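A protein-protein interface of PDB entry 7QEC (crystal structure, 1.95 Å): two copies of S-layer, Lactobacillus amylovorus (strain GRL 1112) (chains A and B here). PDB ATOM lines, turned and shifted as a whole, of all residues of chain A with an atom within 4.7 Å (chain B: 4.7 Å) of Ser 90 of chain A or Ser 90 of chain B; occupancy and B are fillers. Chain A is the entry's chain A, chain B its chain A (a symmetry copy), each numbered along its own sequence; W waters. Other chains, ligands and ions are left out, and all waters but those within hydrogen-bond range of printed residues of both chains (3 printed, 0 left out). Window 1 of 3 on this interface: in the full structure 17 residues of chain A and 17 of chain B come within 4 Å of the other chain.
Phe 89 of chain A touches Pro 107 of chain B, and with the chains exchanged Pro 107 of chain A touches Phe 89 of chain B.
Ser 90 of chain A touches Phe 91 of chain B, and with the chains exchanged Phe 91 of chain A touches Ser 90 of chain B.
Ser 90 of chain A touches Asn 92 of chain B, and with the chains exchanged Asn 92 of chain A touches Ser 90 of chain B.
Ser 90 of chain A touches Pro 107 of chain B, and with the chains exchanged Pro 107 of chain A touches Ser 90 of chain B.
8 positions are printed for both chains.
Of the 11 pairs that touch across the chains among the printed residues, 11 have their exchanged pair printed and touching as well.
Of the 8 printed residues of chain B, 5 touch a printed residue of chain A.
Hydrophobic or aromatic side chains of chain B that line the printed part of chain A: Pro 107.
Along chain B the printed residues that touch a printed residue of chain A span positions 89 to 107.
Of the 8 printed residues of chain A, 5 touch a printed residue of chain B.
Among the printed residues, 11 pairs touch across the chains.
Among the printed residues, no Asp or Glu carboxylate lies within 4 Å of a Lys or Arg side-chain nitrogen of the other chain.
Water W2 lies within hydrogen-bond range of OG of Ser 90 of chain A (2.7 Å), OG of Ser 90 of chain B (2.7 Å), N of Phe 91 of chain A (3.3 Å) and N of Phe 91 of chain B (3.3 Å).
Water W3 lies within hydrogen-bond range of OG1 of Thr 109 of chain A (2.9 Å), OG1 of Thr 109 of chain B (3.1 Å) and O of Pro 107 of chain A (3.2 Å).
Water W1 lies within hydrogen-bond range of the side-chain hydroxyl of Thr 109 of chain B, the side-chain hydroxyl of Thr 109 of chain A and the backbone carbonyl oxygen of Pro 107 of chain B.
The backbone carbonyl oxygen (O) of Phe 91 of chain B sits at hydrogen-bond distance from the backbone NH (N) of Ile 108 of chain B (2.9 Å).
The backbone carbonyl oxygen (O) of Phe 91 of chain A is in hydrogen-bond range of the backbone NH (N) of Ile 108 of chain A (2.9 Å).
Among the printed residues, merely in contact across the chains: Phe 89 of chain A with Asn 92 of chain B, Phe 89 of chain A with Pro 107 of chain B, Ser 90 of chain A with Ser 90 of chain B, Ser 90 of chain A with Phe 91 of chain B, Ser 90 of chain A with Pro 107 of chain B, Phe 91 of chain A with Ser 90 of chain B, Asn 92 of chain A with Phe 89 of chain B, Pro 107 of chain A with Phe 89 of chain B and Pro 107 of chain A with Ser 90 of chain B.
OD1 of Asn 92 of chain B lies close to O of Ser 90 of chain A (2.9 Å).
The side-chain amide oxygen (OD1) of Asn 92 of chain A sits close to the backbone carbonyl oxygen (O) of Ser 90 of chain B (2.9 Å).
Ser 90 of chain A touches just these residues of chain B: Ser 90 (3.7 Å), Phe 91 (3.6 Å), Asn 92 (2.9 Å) and Pro 107 (3.4 Å).
Of chain A, only Ser 90, Phe 91, Asn 92 and Pro 107 come within 4 Å of Ser 90 of chain B.
Printed residues of chain B within 4 Å of Phe 91 of chain A: Ser 90.
Of the printed residues of chain B, Asn 92 of chain A touches Phe 89 and Ser 90.
Of the printed residues of chain A, Asn 92 of chain B touches Phe 89 and Ser 90.
Printed residues of chain A within 4 Å of Phe 91 of chain B: Ser 90 (3.6 Å).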
ATOM      1  N   LEU A  70     -26.179  22.258  36.717  1.00  0.00           N
ATOM      2  CA  LEU A  70     -25.631  20.976  36.276  1.00  0.00           C
ATOM      3  C   LEU A  70     -26.712  19.901  36.181  1.00  0.00           C
ATOM      4  O   LEU A  70     -26.717  19.099  35.235  1.00  0.00           O
ATOM      5  CB  LEU A  70     -24.507  20.529  37.218  1.00  0.00           C
ATOM      6  CG  LEU A  70     -23.329  21.498  37.366  1.00  0.00           C
ATOM      7  CD1 LEU A  70     -22.368  21.002  38.445  1.00  0.00           C
ATOM      8  CD2 LEU A  70     -22.596  21.695  36.047  1.00  0.00           C
ATOM      9  N   PHE A  89     -17.306  20.383  30.321  1.00  0.00           N
ATOM     10  CA  PHE A  89     -18.659  20.862  30.613  1.00  0.00           C
ATOM     11  C   PHE A  89     -18.578  22.359  30.908  1.00  0.00           C
ATOM     12  O   PHE A  89     -17.487  22.919  31.007  1.00  0.00           O
ATOM     13  CB  PHE A  89     -19.312  20.082  31.772  1.00  0.00           C
ATOM     14  CG  PHE A  89     -18.660  20.305  33.132  1.00  0.00           C
ATOM     15  CD1 PHE A  89     -17.582  19.531  33.536  1.00  0.00           C
ATOM     16  CD2 PHE A  89     -19.156  21.262  34.011  1.00  0.00           C
ATOM     17  CE1 PHE A  89     -16.984  19.720  34.785  1.00  0.00           C
ATOM     18  CE2 PHE A  89     -18.564  21.469  35.251  1.00  0.00           C
ATOM     19  CZ  PHE A  89     -17.478  20.692  35.638  1.00  0.00           C
ATOM     20  N   SER A  90     -19.735  23.017  31.033  1.00  0.00           N
ATOM     21  CA  SER A  90     -19.731  24.469  31.256  1.00  0.00           C
ATOM     22  C   SER A  90     -20.787  24.879  32.277  1.00  0.00           C
ATOM     23  O   SER A  90     -21.677  24.107  32.628  1.00  0.00           O
ATOM     24  CB  SER A  90     -19.947  25.247  29.944  1.00  0.00           C
ATOM     25  OG  SER A  90     -21.250  25.026  29.410  1.00  0.00           O
ATOM     26  N   PHE A  91     -20.664  26.121  32.766  1.00  0.00           N
ATOM     27  CA  PHE A  91     -21.664  26.749  33.625  1.00  0.00           C
ATOM     28  C   PHE A  91     -21.512  28.269  33.504  1.00  0.00           C
ATOM     29  O   PHE A  91     -20.523  28.764  32.956  1.00  0.00           O
ATOM     30  CB  PHE A  91     -21.536  26.277  35.088  1.00  0.00           C
ATOM     31  CG  PHE A  91     -20.258  26.712  35.773  1.00  0.00           C
ATOM     32  CD1 PHE A  91     -19.095  25.970  35.638  1.00  0.00           C
ATOM     33  CD2 PHE A  91     -20.236  27.851  36.574  1.00  0.00           C
ATOM     34  CE1 PHE A  91     -17.910  26.353  36.277  1.00  0.00           C
ATOM     35  CE2 PHE A  91     -19.067  28.252  37.206  1.00  0.00           C
ATOM     36  CZ  PHE A  91     -17.892  27.497  37.058  1.00  0.00           C
ATOM     37  N   ASN A  92     -22.503  29.007  34.013  1.00  0.00           N
ATOM     38  CA  ASN A  92     -22.481  30.477  34.002  1.00  0.00           C
ATOM     39  C   ASN A  92     -22.335  31.050  35.414  1.00  0.00           C
ATOM     40  O   ASN A  92     -23.037  30.627  36.344  1.00  0.00           O
ATOM     41  CB  ASN A  92     -23.755  31.052  33.364  1.00  0.00           C
ATOM     42  CG  ASN A  92     -23.949  30.629  31.902  1.00  0.00           C
ATOM     43  OD1 ASN A  92     -24.833  29.835  31.589  1.00  0.00           O
ATOM     44  ND2 ASN A  92     -23.148  31.177  31.011  1.00  0.00           N
ATOM     45  N   PRO A 107     -19.663  32.984  30.937  1.00  0.00           N
ATOM     46  CA  PRO A 107     -19.651  31.533  30.662  1.00  0.00           C
ATOM     47  C   PRO A 107     -18.264  30.953  30.895  1.00  0.00           C
ATOM     48  O   PRO A 107     -17.269  31.485  30.397  1.00  0.00           O
ATOM     49  CB  PRO A 107     -20.040  31.445  29.179  1.00  0.00           C
ATOM     50  CG  PRO A 107     -19.515  32.748  28.582  1.00  0.00           C
ATOM     51  CD  PRO A 107     -19.638  33.791  29.700  1.00  0.00           C
ATOM     52  N   ILE A 108     -18.203  29.838  31.624  1.00  0.00           N
ATOM     53  CA  ILE A 108     -16.936  29.207  31.990  1.00  0.00           C
ATOM     54  C   ILE A 108     -16.936  27.764  31.478  1.00  0.00           C
ATOM     55  O   ILE A 108     -17.819  26.983  31.828  1.00  0.00           O
ATOM     56  CB  ILE A 108     -16.701  29.259  33.506  1.00  0.00           C
ATOM     57  CG1 ILE A 108     -16.436  30.722  33.927  1.00  0.00           C
ATOM     58  CG2 ILE A 108     -15.503  28.368  33.908  1.00  0.00           C
ATOM     59  CD1 ILE A 108     -16.234  30.908  35.384  1.00  0.00           C
ATOM     60  N   THR A 109     -15.942  27.417  30.656  1.00  0.00           N
ATOM     61  CA  THR A 109     -15.734  26.047  30.190  1.00  0.00           C
ATOM     62  C   THR A 109     -14.647  25.350  31.013  1.00  0.00           C
ATOM     63  O   THR A 109     -13.520  25.850  31.110  1.00  0.00           O
ATOM     64  CB  THR A 109     -15.344  26.032  28.709  1.00  0.00           C
ATOM     65  OG1 THR A 109     -16.381  26.646  27.931  1.00  0.00           O
ATOM     66  CG2 THR A 109     -15.156  24.599  28.226  1.00  0.00           C
ATOM     67  N   LEU B  70     -30.900  28.113  31.857  1.00  0.00           N
ATOM     68  CA  LEU B  70     -30.733  29.566  31.809  1.00  0.00           C
ATOM     69  C   LEU B  70     -31.320  30.244  33.046  1.00  0.00           C
ATOM     70  O   LEU B  70     -30.722  31.186  33.586  1.00  0.00           O
ATOM     71  CB  LEU B  70     -31.368  30.129  30.532  1.00  0.00           C
ATOM     72  CG  LEU B  70     -30.833  29.568  29.211  1.00  0.00           C
ATOM     73  CD1 LEU B  70     -31.657  30.096  28.038  1.00  0.00           C
ATOM     74  CD2 LEU B  70     -29.359  29.896  29.019  1.00  0.00           C
ATOM     75  N   PHE B  89     -22.982  33.983  26.757  1.00  0.00           N
ATOM     76  CA  PHE B  89     -23.515  33.055  27.756  1.00  0.00           C
ATOM     77  C   PHE B  89     -23.288  31.632  27.250  1.00  0.00           C
ATOM     78  O   PHE B  89     -22.863  31.432  26.113  1.00  0.00           O
ATOM     79  CB  PHE B  89     -25.002  33.326  28.063  1.00  0.00           C
ATOM     80  CG  PHE B  89     -25.951  33.033  26.905  1.00  0.00           C
ATOM     81  CD1 PHE B  89     -26.220  33.999  25.947  1.00  0.00           C
ATOM     82  CD2 PHE B  89     -26.596  31.804  26.808  1.00  0.00           C
ATOM     83  CE1 PHE B  89     -27.096  33.744  24.889  1.00  0.00           C
ATOM     84  CE2 PHE B  89     -27.461  31.532  25.754  1.00  0.00           C
ATOM     85  CZ  PHE B  89     -27.713  32.508  24.796  1.00  0.00           C
ATOM     86  N   SER B  90     -23.556  30.634  28.100  1.00  0.00           N
ATOM     87  CA  SER B  90     -23.301  29.244  27.700  1.00  0.00           C
ATOM     88  C   SER B  90     -24.419  28.317  28.168  1.00  0.00           C
ATOM     89  O   SER B  90     -25.251  28.679  28.996  1.00  0.00           O
ATOM     90  CB  SER B  90     -21.949  28.737  28.234  1.00  0.00           C
ATOM     91  OG  SER B  90     -21.942  28.649  29.656  1.00  0.00           O
ATOM     92  N   PHE B  91     -24.432  27.101  27.604  1.00  0.00           N
ATOM     93  CA  PHE B  91     -25.319  26.024  28.036  1.00  0.00           C
ATOM     94  C   PHE B  91     -24.688  24.690  27.622  1.00  0.00           C
ATOM     95  O   PHE B  91     -23.734  24.657  26.839  1.00  0.00           O
ATOM     96  CB  PHE B  91     -26.739  26.189  27.458  1.00  0.00           C
ATOM     97  CG  PHE B  91     -26.821  26.038  25.954  1.00  0.00           C
ATOM     98  CD1 PHE B  91     -26.569  27.117  25.121  1.00  0.00           C
ATOM     99  CD2 PHE B  91     -27.177  24.820  25.382  1.00  0.00           C
ATOM    100  CE1 PHE B  91     -26.654  26.995  23.729  1.00  0.00           C
ATOM    101  CE2 PHE B  91     -27.257  24.678  24.004  1.00  0.00           C
ATOM    102  CZ  PHE B  91     -26.993  25.775  23.168  1.00  0.00           C
ATOM    103  N   ASN B  92     -25.224  23.589  28.157  1.00  0.00           N
ATOM    104  CA  ASN B  92     -24.748  22.238  27.828  1.00  0.00           C
ATOM    105  C   ASN B  92     -25.791  21.451  27.031  1.00  0.00           C
ATOM    106  O   ASN B  92     -26.977  21.425  27.393  1.00  0.00           O
ATOM    107  CB  ASN B  92     -24.392  21.444  29.095  1.00  0.00           C
ATOM    108  CG  ASN B  92     -23.272  22.087  29.923  1.00  0.00           C
ATOM    109  OD1 ASN B  92     -23.514  22.614  31.007  1.00  0.00           O
ATOM    110  ND2 ASN B  92     -22.052  22.020  29.430  1.00  0.00           N
ATOM    111  N   PRO B 107     -20.338  21.450  25.944  1.00  0.00           N
ATOM    112  CA  PRO B 107     -20.540  22.856  26.350  1.00  0.00           C
ATOM    113  C   PRO B 107     -20.498  23.776  25.138  1.00  0.00           C
ATOM    114  O   PRO B 107     -19.575  23.700  24.323  1.00  0.00           O
ATOM    115  CB  PRO B 107     -19.357  23.133  27.288  1.00  0.00           C
ATOM    116  CG  PRO B 107     -18.252  22.218  26.769  1.00  0.00           C
ATOM    117  CD  PRO B 107     -18.967  20.975  26.226  1.00  0.00           C
ATOM    118  N   ILE B 108     -21.482  24.671  25.040  1.00  0.00           N
ATOM    119  CA  ILE B 108     -21.613  25.573  23.897  1.00  0.00           C
ATOM    120  C   ILE B 108     -21.603  27.018  24.402  1.00  0.00           C
ATOM    121  O   ILE B 108     -22.436  27.390  25.227  1.00  0.00           O
ATOM    122  CB  ILE B 108     -22.884  25.274  23.091  1.00  0.00           C
ATOM    123  CG1 ILE B 108     -22.724  23.913  22.378  1.00  0.00           C
ATOM    124  CG2 ILE B 108     -23.151  26.387  22.050  1.00  0.00           C
ATOM    125  CD1 ILE B 108     -23.911  23.492  21.596  1.00  0.00           C
ATOM    126  N   THR B 109     -20.664  27.825  23.901  1.00  0.00           N
ATOM    127  CA  THR B 109     -20.609  29.258  24.186  1.00  0.00           C
ATOM    128  C   THR B 109     -21.227  30.066  23.042  1.00  0.00           C
ATOM    129  O   THR B 109     -20.807  29.934  21.886  1.00  0.00           O
ATOM    130  CB  THR B 109     -19.163  29.709  24.410  1.00  0.00           C
ATOM    131  OG1 THR B 109     -18.595  28.983  25.510  1.00  0.00           O
ATOM    132  CG2 THR B 109     -19.117  31.198  24.734  1.00  0.00           C
HETATM  133  O   HOH W   1     -17.812  26.227  25.267  1.00  0.00           O
HETATM  134  O   HOH W   2     -23.215  26.452  30.641  1.00  0.00           O
HETATM  135  O   HOH W   3     -16.779  29.494  27.910  1.00  0.00           O
